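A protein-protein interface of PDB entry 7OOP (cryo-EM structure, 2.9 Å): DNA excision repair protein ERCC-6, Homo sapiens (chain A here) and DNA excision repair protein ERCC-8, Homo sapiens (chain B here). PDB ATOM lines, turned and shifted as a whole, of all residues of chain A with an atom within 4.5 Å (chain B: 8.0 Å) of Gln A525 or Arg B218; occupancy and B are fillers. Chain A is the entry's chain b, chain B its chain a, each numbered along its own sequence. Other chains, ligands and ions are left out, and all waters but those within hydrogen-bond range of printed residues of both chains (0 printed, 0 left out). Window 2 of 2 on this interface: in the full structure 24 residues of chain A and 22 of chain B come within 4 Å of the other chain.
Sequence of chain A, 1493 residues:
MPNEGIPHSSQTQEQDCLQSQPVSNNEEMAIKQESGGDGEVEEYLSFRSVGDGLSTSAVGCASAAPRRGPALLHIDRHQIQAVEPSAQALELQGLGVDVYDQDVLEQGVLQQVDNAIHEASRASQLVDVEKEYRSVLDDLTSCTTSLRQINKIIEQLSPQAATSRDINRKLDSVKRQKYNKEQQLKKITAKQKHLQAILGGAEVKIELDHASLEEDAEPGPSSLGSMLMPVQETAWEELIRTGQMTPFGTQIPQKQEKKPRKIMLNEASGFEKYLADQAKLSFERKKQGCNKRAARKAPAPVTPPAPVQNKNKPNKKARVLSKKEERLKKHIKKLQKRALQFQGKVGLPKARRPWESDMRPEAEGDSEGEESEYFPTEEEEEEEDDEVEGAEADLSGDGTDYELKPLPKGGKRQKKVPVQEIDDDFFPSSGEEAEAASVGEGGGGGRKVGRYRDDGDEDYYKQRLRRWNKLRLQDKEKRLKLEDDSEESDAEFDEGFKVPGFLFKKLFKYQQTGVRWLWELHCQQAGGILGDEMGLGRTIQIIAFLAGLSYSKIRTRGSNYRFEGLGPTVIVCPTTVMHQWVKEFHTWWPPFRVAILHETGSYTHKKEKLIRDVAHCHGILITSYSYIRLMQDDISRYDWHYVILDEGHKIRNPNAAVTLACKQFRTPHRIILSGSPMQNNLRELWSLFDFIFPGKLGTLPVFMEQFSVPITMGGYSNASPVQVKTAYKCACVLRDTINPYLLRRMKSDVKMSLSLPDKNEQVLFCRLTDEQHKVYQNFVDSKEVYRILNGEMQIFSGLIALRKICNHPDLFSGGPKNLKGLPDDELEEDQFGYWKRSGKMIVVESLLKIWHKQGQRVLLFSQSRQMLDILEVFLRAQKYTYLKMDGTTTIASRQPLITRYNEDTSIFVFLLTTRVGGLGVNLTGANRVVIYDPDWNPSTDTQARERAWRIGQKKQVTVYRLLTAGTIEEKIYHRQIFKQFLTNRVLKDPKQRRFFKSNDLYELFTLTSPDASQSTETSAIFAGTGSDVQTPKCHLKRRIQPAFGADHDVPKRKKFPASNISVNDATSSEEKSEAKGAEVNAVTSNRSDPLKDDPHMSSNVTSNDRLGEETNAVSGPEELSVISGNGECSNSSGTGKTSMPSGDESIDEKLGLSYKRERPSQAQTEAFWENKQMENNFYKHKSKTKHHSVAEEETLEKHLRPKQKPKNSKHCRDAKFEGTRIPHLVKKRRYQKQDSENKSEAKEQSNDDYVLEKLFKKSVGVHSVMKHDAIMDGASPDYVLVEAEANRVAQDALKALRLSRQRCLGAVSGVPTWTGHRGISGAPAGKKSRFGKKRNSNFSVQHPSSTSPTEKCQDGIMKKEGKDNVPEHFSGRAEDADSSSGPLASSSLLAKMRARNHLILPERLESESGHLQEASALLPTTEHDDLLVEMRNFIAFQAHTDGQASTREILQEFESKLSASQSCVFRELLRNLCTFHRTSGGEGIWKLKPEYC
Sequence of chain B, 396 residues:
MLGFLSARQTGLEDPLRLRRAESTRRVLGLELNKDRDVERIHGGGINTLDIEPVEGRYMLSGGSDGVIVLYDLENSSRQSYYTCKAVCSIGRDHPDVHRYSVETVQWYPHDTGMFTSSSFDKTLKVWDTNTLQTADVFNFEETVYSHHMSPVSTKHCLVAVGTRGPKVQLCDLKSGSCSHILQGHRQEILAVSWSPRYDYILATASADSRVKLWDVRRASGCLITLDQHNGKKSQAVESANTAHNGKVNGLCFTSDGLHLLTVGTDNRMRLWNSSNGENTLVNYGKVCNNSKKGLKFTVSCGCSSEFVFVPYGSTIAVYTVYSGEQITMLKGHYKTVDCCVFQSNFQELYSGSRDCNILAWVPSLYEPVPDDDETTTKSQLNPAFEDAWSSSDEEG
The guanidinium group (NE) of Arg B218 sits at hydrogen-bond distance from the side-chain amide oxygen (OE1) of Gln A525, 2.9 Å away. N of Ala B219 lies within hydrogen-bond range of O of Gln A525, at 3.1 Å. O of Gln A524 lies close to O of Arg B217, at 3.4 Å.
The backbone NH (N) of Leu B170 lies within hydrogen-bond range of the backbone carbonyl oxygen (O) of His B180, at 3.2 Å. OD2 of Asp B215 is in salt-bridge range of NH2 of Arg B217, at 3.2 Å. The guanidinium group of Arg B218 is in salt-bridge range of the side-chain carboxylate of Asp B215 (3.6 Å). N of Ala A526 lies within hydrogen-bond range of O of Leu A521.
Among the printed residues, merely in contact across the chains: Phe A693 with Ala B219 (3.3 Å), Phe A693 with His B180 (3.4 Å), Gln A524 with Arg B218 (3.5 Å), Phe A693 with Arg B217 (3.6 Å), Phe A693 with Arg B218 (3.8 Å), Pro A668 with Ser B220 (3.9 Å) and Ala A526 with Ala B219 (3.96 Å).
Printed residues of chain B within 4 Å of Gln A524: Arg B217 and Arg B218. Gln A525 touches just these residues of chain B: Arg B218 and Ala B219. Of chain B, only Ala B219 comes within 4 Å of Ala A526. Printed residues of chain A within 4 Å of His B180: Phe A693. Val B216 touches none of the printed residues of chain A. Printed residues of chain A within 4 Å of Arg B217: Gln A524 (3.4 Å) and Phe A693 (3.6 Å). Arg B218 touches just these residues of chain A: Gln A524, Gln A525 and Phe A693. Of the printed residues of chain A, Ala B219 touches Gln A525, Ala A526 and Phe A693. Leu B223 touches none of the printed residues of chain A. The nearest residue of chain B that does not touch Gln A525 is Arg B217 (4.5 Å).
Along chain A the printed residues that touch a printed residue of chain B span positions 524 to 693. Of the 17 printed residues of chain B, 5 touch a printed residue of chain A. Hydrophobic or aromatic side chains of chain B that line the printed part of chain A: His B180 and Ala B219. Among the printed residues, no Asp or Glu carboxylate lies within 4 Å of a Lys or Arg side-chain nitrogen of the other chain.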
ATOM      1  N   LEU A 521      -8.409   7.982 -26.369  1.00  0.00           N
ATOM      2  CA  LEU A 521      -8.497   9.307 -26.960  1.00  0.00           C
ATOM      3  C   LEU A 521      -9.908   9.847 -26.888  1.00  0.00           C
ATOM      4  O   LEU A 521     -10.116  11.010 -26.542  1.00  0.00           O
ATOM      5  CB  LEU A 521      -8.076   9.267 -28.414  1.00  0.00           C
ATOM      6  CG  LEU A 521      -6.656   8.885 -28.776  1.00  0.00           C
ATOM      7  CD1 LEU A 521      -6.501   9.176 -30.229  1.00  0.00           C
ATOM      8  CD2 LEU A 521      -5.619   9.625 -27.967  1.00  0.00           C
ATOM      9  N   HIS A 522     -10.891   9.023 -27.240  1.00  0.00           N
ATOM     10  CA  HIS A 522     -12.263   9.506 -27.259  1.00  0.00           C
ATOM     11  C   HIS A 522     -12.688   9.978 -25.891  1.00  0.00           C
ATOM     12  O   HIS A 522     -13.473  10.919 -25.772  1.00  0.00           O
ATOM     13  CB  HIS A 522     -13.206   8.410 -27.734  1.00  0.00           C
ATOM     14  CG  HIS A 522     -14.639   8.818 -27.735  1.00  0.00           C
ATOM     15  ND1 HIS A 522     -15.171   9.660 -28.686  1.00  0.00           N
ATOM     16  CD2 HIS A 522     -15.649   8.524 -26.888  1.00  0.00           C
ATOM     17  CE1 HIS A 522     -16.451   9.853 -28.433  1.00  0.00           C
ATOM     18  NE2 HIS A 522     -16.766   9.178 -27.344  1.00  0.00           N
ATOM     19  N   CYS A 523     -12.194   9.326 -24.846  1.00  0.00           N
ATOM     20  CA  CYS A 523     -12.460   9.804 -23.499  1.00  0.00           C
ATOM     21  C   CYS A 523     -11.744  11.114 -23.239  1.00  0.00           C
ATOM     22  O   CYS A 523     -12.343  12.061 -22.726  1.00  0.00           O
ATOM     23  CB  CYS A 523     -12.027   8.761 -22.478  1.00  0.00           C
ATOM     24  SG  CYS A 523     -13.221   7.465 -22.234  1.00  0.00           S
ATOM     25  N   GLN A 524     -10.466  11.194 -23.599  1.00  0.00           N
ATOM     26  CA  GLN A 524      -9.747  12.452 -23.478  1.00  0.00           C
ATOM     27  C   GLN A 524     -10.282  13.511 -24.423  1.00  0.00           C
ATOM     28  O   GLN A 524      -9.988  14.689 -24.228  1.00  0.00           O
ATOM     29  CB  GLN A 524      -8.259  12.220 -23.756  1.00  0.00           C
ATOM     30  CG  GLN A 524      -7.517  11.701 -22.567  1.00  0.00           C
ATOM     31  CD  GLN A 524      -6.142  11.183 -22.886  1.00  0.00           C
ATOM     32  OE1 GLN A 524      -5.766  10.092 -22.460  1.00  0.00           O
ATOM     33  NE2 GLN A 524      -5.362  11.978 -23.602  1.00  0.00           N
ATOM     34  N   GLN A 525     -11.083  13.130 -25.411  1.00  0.00           N
ATOM     35  CA  GLN A 525     -11.578  14.058 -26.419  1.00  0.00           C
ATOM     36  C   GLN A 525     -10.429  14.684 -27.196  1.00  0.00           C
ATOM     37  O   GLN A 525     -10.402  15.886 -27.438  1.00  0.00           O
ATOM     38  CB  GLN A 525     -12.467  15.133 -25.804  1.00  0.00           C
ATOM     39  CG  GLN A 525     -13.717  14.593 -25.175  1.00  0.00           C
ATOM     40  CD  GLN A 525     -14.906  15.472 -25.441  1.00  0.00           C
ATOM     41  OE1 GLN A 525     -14.859  16.677 -25.215  1.00  0.00           O
ATOM     42  NE2 GLN A 525     -15.985  14.878 -25.930  1.00  0.00           N
ATOM     43  N   ALA A 526      -9.475  13.857 -27.587  1.00  0.00           N
ATOM     44  CA  ALA A 526      -8.365  14.240 -28.432  1.00  0.00           C
ATOM     45  C   ALA A 526      -8.334  13.332 -29.649  1.00  0.00           C
ATOM     46  O   ALA A 526      -9.041  12.331 -29.721  1.00  0.00           O
ATOM     47  CB  ALA A 526      -7.043  14.151 -27.676  1.00  0.00           C
ATOM     48  N   PRO A 668     -13.718  17.558 -31.679  1.00  0.00           N
ATOM     49  CA  PRO A 668     -12.461  17.153 -31.040  1.00  0.00           C
ATOM     50  C   PRO A 668     -11.869  15.868 -31.569  1.00  0.00           C
ATOM     51  O   PRO A 668     -10.727  15.554 -31.234  1.00  0.00           O
ATOM     52  CB  PRO A 668     -12.858  17.000 -29.574  1.00  0.00           C
ATOM     53  CG  PRO A 668     -14.301  16.778 -29.608  1.00  0.00           C
ATOM     54  CD  PRO A 668     -14.804  17.620 -30.696  1.00  0.00           C
ATOM     55  N   HIS A 669     -12.592  15.118 -32.370  1.00  0.00           N
ATOM     56  CA  HIS A 669     -12.245  13.750 -32.718  1.00  0.00           C
ATOM     57  C   HIS A 669     -11.708  13.758 -34.128  1.00  0.00           C
ATOM     58  O   HIS A 669     -12.465  13.814 -35.095  1.00  0.00           O
ATOM     59  CB  HIS A 669     -13.453  12.843 -32.601  1.00  0.00           C
ATOM     60  CG  HIS A 669     -14.077  12.868 -31.251  1.00  0.00           C
ATOM     61  ND1 HIS A 669     -15.362  13.301 -31.031  1.00  0.00           N
ATOM     62  CD2 HIS A 669     -13.578  12.536 -30.041  1.00  0.00           C
ATOM     63  CE1 HIS A 669     -15.634  13.221 -29.745  1.00  0.00           C
ATOM     64  NE2 HIS A 669     -14.567  12.764 -29.121  1.00  0.00           N
ATOM     65  N   PHE A 693      -4.764  17.499 -33.129  1.00  0.00           N
ATOM     66  CA  PHE A 693      -4.785  18.138 -31.819  1.00  0.00           C
ATOM     67  C   PHE A 693      -4.216  19.539 -32.013  1.00  0.00           C
ATOM     68  O   PHE A 693      -2.990  19.705 -32.037  1.00  0.00           O
ATOM     69  CB  PHE A 693      -3.961  17.339 -30.820  1.00  0.00           C
ATOM     70  CG  PHE A 693      -4.110  17.803 -29.416  1.00  0.00           C
ATOM     71  CD1 PHE A 693      -3.444  18.898 -29.000  1.00  0.00           C
ATOM     72  CD2 PHE A 693      -4.994  17.229 -28.553  1.00  0.00           C
ATOM     73  CE1 PHE A 693      -3.569  19.361 -27.745  1.00  0.00           C
ATOM     74  CE2 PHE A 693      -5.117  17.700 -27.281  1.00  0.00           C
ATOM     75  CZ  PHE A 693      -4.411  18.770 -26.893  1.00  0.00           C
ATOM     76  N   LEU B 170       1.586  25.316 -21.362  1.00  0.00           N
ATOM     77  CA  LEU B 170       1.620  24.198 -20.430  1.00  0.00           C
ATOM     78  C   LEU B 170       2.989  23.547 -20.526  1.00  0.00           C
ATOM     79  O   LEU B 170       3.361  23.046 -21.588  1.00  0.00           O
ATOM     80  CB  LEU B 170       0.522  23.188 -20.746  1.00  0.00           C
ATOM     81  CG  LEU B 170      -0.937  23.611 -20.642  1.00  0.00           C
ATOM     82  CD1 LEU B 170      -1.840  22.440 -20.894  1.00  0.00           C
ATOM     83  CD2 LEU B 170      -1.232  24.168 -19.286  1.00  0.00           C
ATOM     84  N   HIS B 180       2.802  22.674 -25.753  1.00  0.00           N
ATOM     85  CA  HIS B 180       1.353  22.733 -25.673  1.00  0.00           C
ATOM     86  C   HIS B 180       0.908  24.141 -25.354  1.00  0.00           C
ATOM     87  O   HIS B 180       1.488  24.807 -24.498  1.00  0.00           O
ATOM     88  CB  HIS B 180       0.843  21.779 -24.611  1.00  0.00           C
ATOM     89  CG  HIS B 180      -0.625  21.524 -24.693  1.00  0.00           C
ATOM     90  ND1 HIS B 180      -1.555  22.528 -24.613  1.00  0.00           N
ATOM     91  CD2 HIS B 180      -1.325  20.373 -24.783  1.00  0.00           C
ATOM     92  CE1 HIS B 180      -2.767  22.015 -24.692  1.00  0.00           C
ATOM     93  NE2 HIS B 180      -2.655  20.707 -24.796  1.00  0.00           N
ATOM     94  N   ILE B 181      -0.106  24.602 -26.066  1.00  0.00           N
ATOM     95  CA  ILE B 181      -0.670  25.921 -25.864  1.00  0.00           C
ATOM     96  C   ILE B 181      -2.174  25.804 -25.928  1.00  0.00           C
ATOM     97  O   ILE B 181      -2.714  25.007 -26.698  1.00  0.00           O
ATOM     98  CB  ILE B 181      -0.178  26.940 -26.901  1.00  0.00           C
ATOM     99  CG1 ILE B 181      -0.298  26.365 -28.299  1.00  0.00           C
ATOM    100  CG2 ILE B 181       1.235  27.306 -26.609  1.00  0.00           C
ATOM    101  CD1 ILE B 181      -0.191  27.383 -29.357  1.00  0.00           C
ATOM    102  N   LEU B 182      -2.841  26.559 -25.090  1.00  0.00           N
ATOM    103  CA  LEU B 182      -4.282  26.700 -25.123  1.00  0.00           C
ATOM    104  C   LEU B 182      -4.558  28.068 -25.711  1.00  0.00           C
ATOM    105  O   LEU B 182      -4.176  29.081 -25.126  1.00  0.00           O
ATOM    106  CB  LEU B 182      -4.869  26.564 -23.728  1.00  0.00           C
ATOM    107  CG  LEU B 182      -4.415  25.352 -22.924  1.00  0.00           C
ATOM    108  CD1 LEU B 182      -4.613  25.637 -21.474  1.00  0.00           C
ATOM    109  CD2 LEU B 182      -5.190  24.133 -23.315  1.00  0.00           C
ATOM    110  N   TYR B 200      -7.456  18.048 -14.364  1.00  0.00           N
ATOM    111  CA  TYR B 200      -7.146  18.626 -15.661  1.00  0.00           C
ATOM    112  C   TYR B 200      -7.886  19.920 -15.941  1.00  0.00           C
ATOM    113  O   TYR B 200      -7.742  20.466 -17.032  1.00  0.00           O
ATOM    114  CB  TYR B 200      -7.484  17.606 -16.735  1.00  0.00           C
ATOM    115  CG  TYR B 200      -6.573  16.418 -16.753  1.00  0.00           C
ATOM    116  CD1 TYR B 200      -5.338  16.479 -17.367  1.00  0.00           C
ATOM    117  CD2 TYR B 200      -6.935  15.239 -16.123  1.00  0.00           C
ATOM    118  CE1 TYR B 200      -4.514  15.381 -17.406  1.00  0.00           C
ATOM    119  CE2 TYR B 200      -6.109  14.142 -16.141  1.00  0.00           C
ATOM    120  CZ  TYR B 200      -4.893  14.222 -16.773  1.00  0.00           C
ATOM    121  OH  TYR B 200      -4.056  13.132 -16.796  1.00  0.00           O
ATOM    122  N   ILE B 201      -8.658  20.430 -15.004  1.00  0.00           N
ATOM    123  CA  ILE B 201      -9.383  21.671 -15.208  1.00  0.00           C
ATOM    124  C   ILE B 201      -8.450  22.807 -14.845  1.00  0.00           C
ATOM    125  O   ILE B 201      -7.866  22.819 -13.764  1.00  0.00           O
ATOM    126  CB  ILE B 201     -10.665  21.717 -14.369  1.00  0.00           C
ATOM    127  CG1 ILE B 201     -11.647  20.635 -14.811  1.00  0.00           C
ATOM    128  CG2 ILE B 201     -11.320  23.083 -14.452  1.00  0.00           C
ATOM    129  CD1 ILE B 201     -12.193  20.775 -16.213  1.00  0.00           C
ATOM    130  N   TRP B 214     -10.419  25.393 -19.002  1.00  0.00           N
ATOM    131  CA  TRP B 214      -9.934  24.460 -20.004  1.00  0.00           C
ATOM    132  C   TRP B 214      -9.812  23.065 -19.426  1.00  0.00           C
ATOM    133  O   TRP B 214      -9.513  22.889 -18.248  1.00  0.00           O
ATOM    134  CB  TRP B 214      -8.564  24.850 -20.530  1.00  0.00           C
ATOM    135  CG  TRP B 214      -8.369  26.278 -20.811  1.00  0.00           C
ATOM    136  CD1 TRP B 214      -8.094  27.249 -19.924  1.00  0.00           C
ATOM    137  CD2 TRP B 214      -8.424  26.898 -22.084  1.00  0.00           C
ATOM    138  NE1 TRP B 214      -7.969  28.445 -20.555  1.00  0.00           N
ATOM    139  CE2 TRP B 214      -8.172  28.254 -21.891  1.00  0.00           C
ATOM    140  CE3 TRP B 214      -8.663  26.434 -23.373  1.00  0.00           C
ATOM    141  CZ2 TRP B 214      -8.152  29.152 -22.929  1.00  0.00           C
ATOM    142  CZ3 TRP B 214      -8.639  27.315 -24.393  1.00  0.00           C
ATOM    143  CH2 TRP B 214      -8.393  28.666 -24.172  1.00  0.00           C
ATOM    144  N   ASP B 215      -9.995  22.077 -20.282  1.00  0.00           N
ATOM    145  CA  ASP B 215      -9.703  20.687 -19.974  1.00  0.00           C
ATOM    146  C   ASP B 215      -8.515  20.380 -20.863  1.00  0.00           C
ATOM    147  O   ASP B 215      -8.665  20.082 -22.046  1.00  0.00           O
ATOM    148  CB  ASP B 215     -10.886  19.773 -20.243  1.00  0.00           C
ATOM    149  CG  ASP B 215     -10.619  18.335 -19.877  1.00  0.00           C
ATOM    150  OD1 ASP B 215      -9.470  17.989 -19.546  1.00  0.00           O
ATOM    151  OD2 ASP B 215     -11.571  17.531 -19.935  1.00  0.00           O
ATOM    152  N   VAL B 216      -7.328  20.470 -20.276  1.00  0.00           N
ATOM    153  CA  VAL B 216      -6.098  20.415 -21.037  1.00  0.00           C
ATOM    154  C   VAL B 216      -5.968  19.103 -21.780  1.00  0.00           C
ATOM    155  O   VAL B 216      -5.203  19.009 -22.738  1.00  0.00           O
ATOM    156  CB  VAL B 216      -4.915  20.642 -20.098  1.00  0.00           C
ATOM    157  CG1 VAL B 216      -5.067  21.970 -19.396  1.00  0.00           C
ATOM    158  CG2 VAL B 216      -4.803  19.515 -19.093  1.00  0.00           C
ATOM    159  N   ARG B 217      -6.676  18.071 -21.336  1.00  0.00           N
ATOM    160  CA  ARG B 217      -6.788  16.854 -22.119  1.00  0.00           C
ATOM    161  C   ARG B 217      -7.514  17.119 -23.424  1.00  0.00           C
ATOM    162  O   ARG B 217      -7.135  16.591 -24.471  1.00  0.00           O
ATOM    163  CB  ARG B 217      -7.547  15.802 -21.321  1.00  0.00           C
ATOM    164  CG  ARG B 217      -6.704  14.885 -20.475  1.00  0.00           C
ATOM    165  CD  ARG B 217      -7.583  13.970 -19.622  1.00  0.00           C
ATOM    166  NE  ARG B 217      -8.465  14.715 -18.727  1.00  0.00           N
ATOM    167  CZ  ARG B 217      -9.795  14.634 -18.683  1.00  0.00           C
ATOM    168  NH1 ARG B 217     -10.492  13.843 -19.489  1.00  0.00           N
ATOM    169  NH2 ARG B 217     -10.446  15.378 -17.804  1.00  0.00           N
ATOM    170  N   ARG B 218      -8.568  17.921 -23.372  1.00  0.00           N
ATOM    171  CA  ARG B 218      -9.430  18.148 -24.519  1.00  0.00           C
ATOM    172  C   ARG B 218      -8.682  18.897 -25.601  1.00  0.00           C
ATOM    173  O   ARG B 218      -7.788  19.698 -25.327  1.00  0.00           O
ATOM    174  CB  ARG B 218     -10.657  18.946 -24.096  1.00  0.00           C
ATOM    175  CG  ARG B 218     -11.783  18.967 -25.110  1.00  0.00           C
ATOM    176  CD  ARG B 218     -13.159  19.177 -24.490  1.00  0.00           C
ATOM    177  NE  ARG B 218     -13.432  18.301 -23.357  1.00  0.00           N
ATOM    178  CZ  ARG B 218     -14.596  18.243 -22.717  1.00  0.00           C
ATOM    179  NH1 ARG B 218     -15.621  18.999 -23.097  1.00  0.00           N
ATOM    180  NH2 ARG B 218     -14.743  17.411 -21.697  1.00  0.00           N
ATOM    181  N   ALA B 219      -9.080  18.656 -26.842  1.00  0.00           N
ATOM    182  CA  ALA B 219      -8.434  19.239 -28.004  1.00  0.00           C
ATOM    183  C   ALA B 219      -9.302  20.293 -28.667  1.00  0.00           C
ATOM    184  O   ALA B 219      -9.082  20.624 -29.828  1.00  0.00           O
ATOM    185  CB  ALA B 219      -8.114  18.145 -29.015  1.00  0.00           C
ATOM    186  N   SER B 220     -10.271  20.847 -27.947  1.00  0.00           N
ATOM    187  CA  SER B 220     -11.312  21.637 -28.589  1.00  0.00           C
ATOM    188  C   SER B 220     -11.629  22.918 -27.831  1.00  0.00           C
ATOM    189  O   SER B 220     -12.797  23.301 -27.721  1.00  0.00           O
ATOM    190  CB  SER B 220     -12.581  20.812 -28.756  1.00  0.00           C
ATOM    191  OG  SER B 220     -13.132  20.469 -27.502  1.00  0.00           O
ATOM    192  N   GLY B 221     -10.627  23.585 -27.307  1.00  0.00           N
ATOM    193  CA  GLY B 221     -10.847  24.898 -26.754  1.00  0.00           C
ATOM    194  C   GLY B 221     -11.418  24.861 -25.349  1.00  0.00           C
ATOM    195  O   GLY B 221     -11.546  23.817 -24.710  1.00  0.00           O
ATOM    196  N   CYS B 222     -11.771  26.046 -24.873  1.00  0.00           N
ATOM    197  CA  CYS B 222     -12.203  26.202 -23.497  1.00  0.00           C
ATOM    198  C   CYS B 222     -13.543  25.521 -23.265  1.00  0.00           C
ATOM    199  O   CYS B 222     -14.401  25.489 -24.146  1.00  0.00           O
ATOM    200  CB  CYS B 222     -12.276  27.684 -23.149  1.00  0.00           C
ATOM    201  SG  CYS B 222     -13.540  28.628 -24.003  1.00  0.00           S
ATOM    202  N   LEU B 223     -13.706  24.939 -22.075  1.00  0.00           N
ATOM    203  CA  LEU B 223     -14.999  24.379 -21.694  1.00  0.00           C
ATOM    204  C   LEU B 223     -16.034  25.467 -21.549  1.00  0.00           C
ATOM    205  O   LEU B 223     -17.119  25.401 -22.133  1.00  0.00           O
ATOM    206  CB  LEU B 223     -14.883  23.627 -20.371  1.00  0.00           C
ATOM    207  CG  LEU B 223     -14.427  22.178 -20.368  1.00  0.00           C
ATOM    208  CD1 LEU B 223     -15.443  21.259 -20.990  1.00  0.00           C
ATOM    209  CD2 LEU B 223     -13.142  22.060 -21.110  1.00  0.00           C
ATOM    210  N   ILE B 224     -15.715  26.467 -20.745  1.00  0.00           N
ATOM    211  CA  ILE B 224     -16.656  27.488 -20.343  1.00  0.00           C
ATOM    212  C   ILE B 224     -15.922  28.808 -20.355  1.00  0.00           C
ATOM    213  O   ILE B 224     -14.730  28.885 -20.055  1.00  0.00           O
ATOM    214  CB  ILE B 224     -17.253  27.216 -18.953  1.00  0.00           C
ATOM    215  CG1 ILE B 224     -18.044  25.913 -18.975  1.00  0.00           C
ATOM    216  CG2 ILE B 224     -18.176  28.352 -18.553  1.00  0.00           C
ATOM    217  CD1 ILE B 224     -18.454  25.403 -17.635  1.00  0.00           C
